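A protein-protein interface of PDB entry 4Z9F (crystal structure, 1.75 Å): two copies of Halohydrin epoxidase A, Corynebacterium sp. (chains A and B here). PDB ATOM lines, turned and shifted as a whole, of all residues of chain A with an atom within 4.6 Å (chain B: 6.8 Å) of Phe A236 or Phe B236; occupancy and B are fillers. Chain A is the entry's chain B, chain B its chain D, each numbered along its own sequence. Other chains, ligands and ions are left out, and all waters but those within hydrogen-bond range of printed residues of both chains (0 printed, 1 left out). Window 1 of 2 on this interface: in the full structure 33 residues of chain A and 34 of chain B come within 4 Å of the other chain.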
ATOM      1  N   TYR A 173       1.140 -16.893  22.631  1.00  0.00           N
ATOM      2  CA  TYR A 173       2.322 -16.324  22.004  1.00  0.00           C
ATOM      3  C   TYR A 173       1.934 -15.854  20.612  1.00  0.00           C
ATOM      4  O   TYR A 173       0.953 -16.327  20.039  1.00  0.00           O
ATOM      5  CB  TYR A 173       3.479 -17.328  21.880  1.00  0.00           C
ATOM      6  CG  TYR A 173       3.780 -18.124  23.128  1.00  0.00           C
ATOM      7  CD1 TYR A 173       4.750 -17.693  24.030  1.00  0.00           C
ATOM      8  CD2 TYR A 173       3.117 -19.327  23.386  1.00  0.00           C
ATOM      9  CE1 TYR A 173       5.055 -18.427  25.176  1.00  0.00           C
ATOM     10  CE2 TYR A 173       3.411 -20.073  24.545  1.00  0.00           C
ATOM     11  CZ  TYR A 173       4.381 -19.605  25.427  1.00  0.00           C
ATOM     12  OH  TYR A 173       4.686 -20.325  26.572  1.00  0.00           O
ATOM     13  N   ALA A 174       2.693 -14.896  20.093  1.00  0.00           N
ATOM     14  CA  ALA A 174       2.555 -14.497  18.699  1.00  0.00           C
ATOM     15  C   ALA A 174       3.913 -14.616  18.028  1.00  0.00           C
ATOM     16  O   ALA A 174       4.929 -14.163  18.569  1.00  0.00           O
ATOM     17  CB  ALA A 174       1.999 -13.072  18.548  1.00  0.00           C
ATOM     18  N   ILE A 175       3.928 -15.223  16.848  1.00  0.00           N
ATOM     19  CA  ILE A 175       5.123 -15.304  16.020  1.00  0.00           C
ATOM     20  C   ILE A 175       4.895 -14.403  14.824  1.00  0.00           C
ATOM     21  O   ILE A 175       3.808 -14.424  14.232  1.00  0.00           O
ATOM     22  CB  ILE A 175       5.415 -16.741  15.559  1.00  0.00           C
ATOM     23  CG1 ILE A 175       5.586 -17.671  16.764  1.00  0.00           C
ATOM     24  CG2 ILE A 175       6.646 -16.770  14.673  1.00  0.00           C
ATOM     25  CD1 ILE A 175       5.601 -19.142  16.380  1.00  0.00           C
ATOM     26  N   GLY A 176       5.906 -13.599  14.481  1.00  0.00           N
ATOM     27  CA  GLY A 176       5.759 -12.666  13.389  1.00  0.00           C
ATOM     28  C   GLY A 176       6.787 -12.891  12.301  1.00  0.00           C
ATOM     29  O   GLY A 176       7.861 -12.299  12.308  1.00  0.00           O
ATOM     30  N   LEU A 223       7.891 -23.811  21.980  1.00  0.00           N
ATOM     31  CA  LEU A 223       6.803 -23.155  22.702  1.00  0.00           C
ATOM     32  C   LEU A 223       5.794 -24.177  23.211  1.00  0.00           C
ATOM     33  O   LEU A 223       5.350 -24.098  24.361  1.00  0.00           O
ATOM     34  CB  LEU A 223       6.112 -22.109  21.815  1.00  0.00           C
ATOM     35  CG  LEU A 223       7.002 -20.941  21.385  1.00  0.00           C
ATOM     36  CD1 LEU A 223       6.243 -19.988  20.437  1.00  0.00           C
ATOM     37  CD2 LEU A 223       7.547 -20.184  22.610  1.00  0.00           C
ATOM     38  N   ILE A 231       8.276 -16.859  29.167  1.00  0.00           N
ATOM     39  CA  ILE A 231       8.343 -15.953  28.014  1.00  0.00           C
ATOM     40  C   ILE A 231       6.935 -15.747  27.444  1.00  0.00           C
ATOM     41  O   ILE A 231       6.767 -15.145  26.374  1.00  0.00           O
ATOM     42  CB  ILE A 231       9.325 -16.453  26.931  1.00  0.00           C
ATOM     43  CG1 ILE A 231       8.869 -17.769  26.310  1.00  0.00           C
ATOM     44  CG2 ILE A 231      10.742 -16.623  27.476  1.00  0.00           C
ATOM     45  CD1 ILE A 231       9.841 -18.278  25.243  1.00  0.00           C
ATOM     46  N   GLN A 234       4.096 -12.665  24.517  1.00  0.00           N
ATOM     47  CA  GLN A 234       4.826 -11.676  23.742  1.00  0.00           C
ATOM     48  C   GLN A 234       4.920 -12.131  22.299  1.00  0.00           C
ATOM     49  O   GLN A 234       4.511 -13.240  21.936  1.00  0.00           O
ATOM     50  CB  GLN A 234       6.235 -11.396  24.309  1.00  0.00           C
ATOM     51  CG  GLN A 234       7.243 -12.507  24.104  1.00  0.00           C
ATOM     52  CD  GLN A 234       8.549 -12.272  24.861  1.00  0.00           C
ATOM     53  OE1 GLN A 234       9.305 -11.344  24.556  1.00  0.00           O
ATOM     54  NE2 GLN A 234       8.816 -13.120  25.852  1.00  0.00           N
ATOM     55  N   PHE A 235       5.448 -11.217  21.490  1.00  0.00           N
ATOM     56  CA  PHE A 235       5.652 -11.369  20.059  1.00  0.00           C
ATOM     57  C   PHE A 235       7.102 -11.758  19.801  1.00  0.00           C
ATOM     58  O   PHE A 235       8.028 -11.180  20.397  1.00  0.00           O
ATOM     59  CB  PHE A 235       5.278 -10.044  19.381  1.00  0.00           C
ATOM     60  CG  PHE A 235       5.616  -9.944  17.924  1.00  0.00           C
ATOM     61  CD1 PHE A 235       4.635 -10.161  16.957  1.00  0.00           C
ATOM     62  CD2 PHE A 235       6.867  -9.531  17.517  1.00  0.00           C
ATOM     63  CE1 PHE A 235       4.939 -10.008  15.607  1.00  0.00           C
ATOM     64  CE2 PHE A 235       7.168  -9.392  16.179  1.00  0.00           C
ATOM     65  CZ  PHE A 235       6.200  -9.628  15.229  1.00  0.00           C
ATOM     66  N   PHE A 236       7.297 -12.765  18.950  1.00  0.00           N
ATOM     67  CA  PHE A 236       8.620 -13.198  18.529  1.00  0.00           C
ATOM     68  C   PHE A 236       8.784 -12.915  17.045  1.00  0.00           C
ATOM     69  O   PHE A 236       8.038 -13.462  16.225  1.00  0.00           O
ATOM     70  CB  PHE A 236       8.820 -14.685  18.802  1.00  0.00           C
ATOM     71  CG  PHE A 236       8.612 -15.049  20.237  1.00  0.00           C
ATOM     72  CD1 PHE A 236       7.561 -15.867  20.608  1.00  0.00           C
ATOM     73  CD2 PHE A 236       9.439 -14.526  21.220  1.00  0.00           C
ATOM     74  CE1 PHE A 236       7.349 -16.193  21.930  1.00  0.00           C
ATOM     75  CE2 PHE A 236       9.235 -14.844  22.547  1.00  0.00           C
ATOM     76  CZ  PHE A 236       8.185 -15.679  22.903  1.00  0.00           C
ATOM     77  N   ALA A 237       9.753 -12.075  16.709  1.00  0.00           N
ATOM     78  CA  ALA A 237      10.104 -11.905  15.308  1.00  0.00           C
ATOM     79  C   ALA A 237      10.743 -13.186  14.794  1.00  0.00           C
ATOM     80  O   ALA A 237      11.557 -13.817  15.479  1.00  0.00           O
ATOM     81  CB  ALA A 237      11.051 -10.726  15.121  1.00  0.00           C
ATOM     82  N   PHE A 238      10.329 -13.595  13.592  1.00  0.00           N
ATOM     83  CA  PHE A 238      10.910 -14.741  12.885  1.00  0.00           C
ATOM     84  C   PHE A 238      11.305 -14.234  11.498  1.00  0.00           C
ATOM     85  O   PHE A 238      10.652 -14.528  10.504  1.00  0.00           O
ATOM     86  CB  PHE A 238       9.926 -15.912  12.810  1.00  0.00           C
ATOM     87  CG  PHE A 238      10.544 -17.193  12.337  1.00  0.00           C
ATOM     88  CD1 PHE A 238      11.070 -18.102  13.238  1.00  0.00           C
ATOM     89  CD2 PHE A 238      10.594 -17.493  10.980  1.00  0.00           C
ATOM     90  CE1 PHE A 238      11.626 -19.288  12.800  1.00  0.00           C
ATOM     91  CE2 PHE A 238      11.151 -18.675  10.534  1.00  0.00           C
ATOM     92  CZ  PHE A 238      11.673 -19.577  11.449  1.00  0.00           C
ATOM     93  N   THR B 133      20.017  -9.353  30.187  1.00  0.00           N
ATOM     94  CA  THR B 133      19.884  -7.939  30.508  1.00  0.00           C
ATOM     95  C   THR B 133      18.870  -7.800  31.635  1.00  0.00           C
ATOM     96  O   THR B 133      19.106  -8.318  32.731  1.00  0.00           O
ATOM     97  CB  THR B 133      19.517  -7.113  29.268  1.00  0.00           C
ATOM     98  OG1 THR B 133      18.239  -7.504  28.745  1.00  0.00           O
ATOM     99  CG2 THR B 133      20.579  -7.298  28.166  1.00  0.00           C
ATOM    100  N   SER B 134      17.734  -7.159  31.374  1.00  0.00           N
ATOM    101  CA  SER B 134      16.693  -6.976  32.375  1.00  0.00           C
ATOM    102  C   SER B 134      15.433  -6.489  31.671  1.00  0.00           C
ATOM    103  O   SER B 134      15.487  -6.000  30.540  1.00  0.00           O
ATOM    104  CB  SER B 134      17.129  -5.982  33.462  1.00  0.00           C
ATOM    105  OG  SER B 134      16.015  -5.535  34.217  1.00  0.00           O
ATOM    106  N   LEU B 172      23.113 -13.162  17.914  1.00  0.00           N
ATOM    107  CA  LEU B 172      23.008 -12.425  19.172  1.00  0.00           C
ATOM    108  C   LEU B 172      21.567 -12.367  19.666  1.00  0.00           C
ATOM    109  O   LEU B 172      20.633 -12.184  18.882  1.00  0.00           O
ATOM    110  CB  LEU B 172      23.551 -10.998  19.019  1.00  0.00           C
ATOM    111  CG  LEU B 172      25.038 -10.804  19.334  1.00  0.00           C
ATOM    112  CD1 LEU B 172      25.912 -11.693  18.455  1.00  0.00           C
ATOM    113  CD2 LEU B 172      25.431  -9.351  19.176  1.00  0.00           C
ATOM    114  N   TYR B 173      21.386 -12.484  20.984  1.00  0.00           N
ATOM    115  CA  TYR B 173      20.051 -12.403  21.572  1.00  0.00           C
ATOM    116  C   TYR B 173      20.152 -11.665  22.895  1.00  0.00           C
ATOM    117  O   TYR B 173      21.211 -11.662  23.524  1.00  0.00           O
ATOM    118  CB  TYR B 173      19.450 -13.792  21.839  1.00  0.00           C
ATOM    119  CG  TYR B 173      19.528 -14.762  20.677  1.00  0.00           C
ATOM    120  CD1 TYR B 173      18.466 -14.900  19.788  1.00  0.00           C
ATOM    121  CD2 TYR B 173      20.664 -15.540  20.466  1.00  0.00           C
ATOM    122  CE1 TYR B 173      18.533 -15.791  18.726  1.00  0.00           C
ATOM    123  CE2 TYR B 173      20.735 -16.433  19.407  1.00  0.00           C
ATOM    124  CZ  TYR B 173      19.658 -16.557  18.542  1.00  0.00           C
ATOM    125  OH  TYR B 173      19.728 -17.439  17.479  1.00  0.00           O
ATOM    126  N   ALA B 174      19.052 -11.039  23.312  1.00  0.00           N
ATOM    127  CA  ALA B 174      18.970 -10.425  24.629  1.00  0.00           C
ATOM    128  C   ALA B 174      17.787 -11.027  25.375  1.00  0.00           C
ATOM    129  O   ALA B 174      16.677 -11.102  24.835  1.00  0.00           O
ATOM    130  CB  ALA B 174      18.825  -8.900  24.531  1.00  0.00           C
ATOM    131  N   ILE B 175      18.026 -11.459  26.613  1.00  0.00           N
ATOM    132  CA  ILE B 175      16.970 -11.920  27.507  1.00  0.00           C
ATOM    133  C   ILE B 175      16.791 -10.862  28.582  1.00  0.00           C
ATOM    134  O   ILE B 175      17.779 -10.381  29.153  1.00  0.00           O
ATOM    135  CB  ILE B 175      17.295 -13.292  28.119  1.00  0.00           C
ATOM    136  CG1 ILE B 175      17.565 -14.308  27.005  1.00  0.00           C
ATOM    137  CG2 ILE B 175      16.130 -13.764  28.994  1.00  0.00           C
ATOM    138  CD1 ILE B 175      18.085 -15.658  27.487  1.00  0.00           C
ATOM    139  N   GLY B 176      15.537 -10.484  28.847  1.00  0.00           N
ATOM    140  CA  GLY B 176      15.241  -9.464  29.824  1.00  0.00           C
ATOM    141  C   GLY B 176      14.369  -9.984  30.953  1.00  0.00           C
ATOM    142  O   GLY B 176      13.137  -9.903  30.904  1.00  0.00           O
ATOM    143  N   PRO B 177      14.990 -10.518  31.998  1.00  0.00           N
ATOM    144  CA  PRO B 177      14.220 -11.152  33.069  1.00  0.00           C
ATOM    145  C   PRO B 177      13.662 -10.163  34.076  1.00  0.00           C
ATOM    146  O   PRO B 177      14.235  -9.103  34.340  1.00  0.00           O
ATOM    147  CB  PRO B 177      15.243 -12.071  33.749  1.00  0.00           C
ATOM    148  CG  PRO B 177      16.540 -11.861  33.019  1.00  0.00           C
ATOM    149  CD  PRO B 177      16.438 -10.619  32.244  1.00  0.00           C
ATOM    150  N   LEU B 219      15.330 -21.826  27.955  1.00  0.00           N
ATOM    151  CA  LEU B 219      15.450 -20.781  26.940  1.00  0.00           C
ATOM    152  C   LEU B 219      16.885 -20.646  26.464  1.00  0.00           C
ATOM    153  O   LEU B 219      17.139 -20.414  25.277  1.00  0.00           O
ATOM    154  CB  LEU B 219      14.960 -19.445  27.489  1.00  0.00           C
ATOM    155  CG  LEU B 219      15.021 -18.240  26.547  1.00  0.00           C
ATOM    156  CD1 LEU B 219      14.078 -18.444  25.349  1.00  0.00           C
ATOM    157  CD2 LEU B 219      14.666 -16.966  27.298  1.00  0.00           C
ATOM    158  N   LEU B 223      18.119 -21.355  22.507  1.00  0.00           N
ATOM    159  CA  LEU B 223      18.863 -20.397  21.692  1.00  0.00           C
ATOM    160  C   LEU B 223      20.229 -20.955  21.289  1.00  0.00           C
ATOM    161  O   LEU B 223      20.630 -20.856  20.124  1.00  0.00           O
ATOM    162  CB  LEU B 223      19.014 -19.080  22.448  1.00  0.00           C
ATOM    163  CG  LEU B 223      17.714 -18.361  22.817  1.00  0.00           C
ATOM    164  CD1 LEU B 223      18.037 -17.110  23.599  1.00  0.00           C
ATOM    165  CD2 LEU B 223      16.920 -18.010  21.576  1.00  0.00           C
ATOM    166  N   ILE B 231      15.069 -16.155  14.645  1.00  0.00           N
ATOM    167  CA  ILE B 231      14.617 -15.248  15.702  1.00  0.00           C
ATOM    168  C   ILE B 231      15.811 -14.452  16.244  1.00  0.00           C
ATOM    169  O   ILE B 231      15.689 -13.742  17.249  1.00  0.00           O
ATOM    170  CB  ILE B 231      13.872 -15.993  16.832  1.00  0.00           C
ATOM    171  CG1 ILE B 231      14.816 -16.920  17.609  1.00  0.00           C
ATOM    172  CG2 ILE B 231      12.674 -16.790  16.294  1.00  0.00           C
ATOM    173  CD1 ILE B 231      14.124 -17.746  18.678  1.00  0.00           C
ATOM    174  N   VAL B 232      16.946 -14.504  15.535  1.00  0.00           N
ATOM    175  CA  VAL B 232      18.161 -13.808  15.959  1.00  0.00           C
ATOM    176  C   VAL B 232      17.917 -12.299  16.082  1.00  0.00           C
ATOM    177  O   VAL B 232      17.091 -11.713  15.372  1.00  0.00           O
ATOM    178  CB  VAL B 232      19.304 -14.096  14.965  1.00  0.00           C
ATOM    179  CG1 VAL B 232      18.936 -13.599  13.568  1.00  0.00           C
ATOM    180  CG2 VAL B 232      20.619 -13.448  15.398  1.00  0.00           C
ATOM    181  N   GLY B 233      18.631 -11.667  17.009  1.00  0.00           N
ATOM    182  CA  GLY B 233      18.725 -10.221  17.021  1.00  0.00           C
ATOM    183  C   GLY B 233      17.627  -9.474  17.741  1.00  0.00           C
ATOM    184  O   GLY B 233      17.404  -8.295  17.439  1.00  0.00           O
ATOM    185  N   GLN B 234      16.935 -10.103  18.687  1.00  0.00           N
ATOM    186  CA  GLN B 234      15.815  -9.430  19.328  1.00  0.00           C
ATOM    187  C   GLN B 234      15.854  -9.672  20.823  1.00  0.00           C
ATOM    188  O   GLN B 234      16.653 -10.454  21.341  1.00  0.00           O
ATOM    189  CB  GLN B 234      14.453  -9.880  18.755  1.00  0.00           C
ATOM    190  CG  GLN B 234      14.001 -11.252  19.221  1.00  0.00           C
ATOM    191  CD  GLN B 234      12.767 -11.742  18.467  1.00  0.00           C
ATOM    192  OE1 GLN B 234      11.670 -11.193  18.606  1.00  0.00           O
ATOM    193  NE2 GLN B 234      12.949 -12.772  17.661  1.00  0.00           N
ATOM    194  N   PHE B 235      14.969  -8.965  21.503  1.00  0.00           N
ATOM    195  CA  PHE B 235      14.823  -9.018  22.949  1.00  0.00           C
ATOM    196  C   PHE B 235      13.706  -9.985  23.305  1.00  0.00           C
ATOM    197  O   PHE B 235      12.632  -9.947  22.692  1.00  0.00           O
ATOM    198  CB  PHE B 235      14.522  -7.613  23.461  1.00  0.00           C
ATOM    199  CG  PHE B 235      14.198  -7.531  24.925  1.00  0.00           C
ATOM    200  CD1 PHE B 235      15.174  -7.167  25.837  1.00  0.00           C
ATOM    201  CD2 PHE B 235      12.909  -7.759  25.379  1.00  0.00           C
ATOM    202  CE1 PHE B 235      14.869  -7.055  27.189  1.00  0.00           C
ATOM    203  CE2 PHE B 235      12.602  -7.650  26.715  1.00  0.00           C
ATOM    204  CZ  PHE B 235      13.590  -7.293  27.626  1.00  0.00           C
ATOM    205  N   PHE B 236      13.953 -10.841  24.294  1.00  0.00           N
ATOM    206  CA  PHE B 236      12.945 -11.762  24.811  1.00  0.00           C
ATOM    207  C   PHE B 236      12.667 -11.407  26.261  1.00  0.00           C
ATOM    208  O   PHE B 236      13.569 -11.472  27.101  1.00  0.00           O
ATOM    209  CB  PHE B 236      13.398 -13.222  24.729  1.00  0.00           C
ATOM    210  CG  PHE B 236      13.789 -13.657  23.356  1.00  0.00           C
ATOM    211  CD1 PHE B 236      15.123 -13.824  23.027  1.00  0.00           C
ATOM    212  CD2 PHE B 236      12.834 -13.896  22.389  1.00  0.00           C
ATOM    213  CE1 PHE B 236      15.503 -14.220  21.760  1.00  0.00           C
ATOM    214  CE2 PHE B 236      13.216 -14.287  21.107  1.00  0.00           C
ATOM    215  CZ  PHE B 236      14.552 -14.447  20.797  1.00  0.00           C
ATOM    216  N   ALA B 237      11.430 -11.039  26.555  1.00  0.00           N
ATOM    217  CA  ALA B 237      11.054 -10.853  27.949  1.00  0.00           C
ATOM    218  C   ALA B 237      11.013 -12.212  28.639  1.00  0.00           C
ATOM    219  O   ALA B 237      10.572 -13.206  28.054  1.00  0.00           O
ATOM    220  CB  ALA B 237       9.703 -10.145  28.044  1.00  0.00           C
ATOM    221  N   PHE B 238      11.511 -12.270  29.887  1.00  0.00           N
ATOM    222  CA  PHE B 238      11.416 -13.478  30.724  1.00  0.00           C
ATOM    223  C   PHE B 238      10.805 -13.036  32.055  1.00  0.00           C
ATOM    224  O   PHE B 238      11.481 -12.930  33.079  1.00  0.00           O
ATOM    225  CB  PHE B 238      12.783 -14.153  30.905  1.00  0.00           C
ATOM    226  CG  PHE B 238      12.724 -15.515  31.577  1.00  0.00           C
ATOM    227  CD1 PHE B 238      12.624 -16.675  30.826  1.00  0.00           C
ATOM    228  CD2 PHE B 238      12.787 -15.621  32.961  1.00  0.00           C
ATOM    229  CE1 PHE B 238      12.581 -17.927  31.448  1.00  0.00           C
ATOM    230  CE2 PHE B 238      12.756 -16.855  33.590  1.00  0.00           C
ATOM    231  CZ  PHE B 238      12.644 -18.011  32.835  1.00  0.00           C
ATOM    232  N   THR B 239       9.515 -12.725  32.014  1.00  0.00           N
ATOM    233  CA  THR B 239       8.862 -11.983  33.079  1.00  0.00           C
ATOM    234  C   THR B 239       7.533 -12.587  33.512  1.00  0.00           C
ATOM    235  O   THR B 239       6.841 -11.975  34.330  1.00  0.00           O
ATOM    236  CB  THR B 239       8.617 -10.520  32.655  1.00  0.00           C
ATOM    237  OG1 THR B 239       7.559 -10.458  31.672  1.00  0.00           O
ATOM    238  CG2 THR B 239       9.883  -9.877  32.090  1.00  0.00           C
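Hydrophobic or aromatic side chains of chain A within 4 Å of the printed part of chain B: Ile A231, Phe A236, Ala A237 and Phe A238. Among the printed residues, no Asp or Glu carboxylate lies within 4 Å of a Lys or Arg side-chain nitrogen of the other chain.
The backbone NH (N) of Phe B236 lies within hydrogen-bond range of the backbone carbonyl oxygen (O) of Ala B174, 2.8 Å away. N of Gly B176 lies within hydrogen-bond range of O of Phe B236 (2.8 Å). The backbone carbonyl oxygen (O) of Ile A231 lies within hydrogen-bond range of the side-chain amide nitrogen (NE2) of Gln A234, at 2.9 Å. The backbone NH of Phe B238 is in hydrogen-bond range of the backbone carbonyl oxygen of Gly B176 (3.0 Å). The backbone NH of Ala A174 is in hydrogen-bond range of the backbone carbonyl oxygen of Gln A234 (3.1 Å). The backbone carbonyl oxygen (O) of Ile B231 lies within hydrogen-bond range of the side-chain amide nitrogen (NE2) of Gln B234.
Ile A231 touches Leu B219 (CG2 to CD2, 3.9 Å). Ala B237 touches Ile A231. Phe B238 touches Ile A231 (CD1 to CG2, 3.8 Å). CA of Phe B236 touches OE1 of Gln A234, 3.7 Å away. CA of Phe A236 touches OE1 of Gln B234, at 3.7 Å. Phe A236 touches Phe B236 (CD2 to CD2, 3.6 Å). Ala A237 touches Ile B231. Phe A238 touches Ile B231.
The backbone carbonyl oxygen (O) of Ala A237 sits at hydrogen-bond distance from the side-chain amide nitrogen (NE2) of Gln B234 (2.8 Å). The backbone carbonyl oxygen (O) of Ala B237 is in hydrogen-bond range of the side-chain amide nitrogen (NE2) of Gln A234.
Ile A231 touches Phe B238, and with the chains exchanged Phe A238 touches Ile B231. Gln A234 touches Phe B236, and with the chains exchanged Phe A236 touches Gln B234. Gln A234 touches Ala B237, and with the chains exchanged Ala A237 touches Gln B234. Phe A236 touches its own counterpart, Phe B236.
Of the printed residues of chain B, Ile A231 touches Leu B219 (3.9 Å), Ala B237 (3.5 Å) and Phe B238 (3.8 Å). Of chain B, only Gln B234 (3.7 Å) and Phe B236 (3.6 Å) come within 4 Å of Phe A236. Of the printed residues of chain B, Ala A237 touches Ile B231 and Gln B234. Of the printed residues of chain B, Phe A238 touches Ile B231 (3.7 Å). Of the printed residues of chain A, Leu B219 touches Ile A231. Phe B236 touches just these residues of chain A: Gln A234 and Phe A236. Of the printed residues of chain A, Ala B237 touches Ile A231 (3.5 Å) and Gln A234 (2.8 Å).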
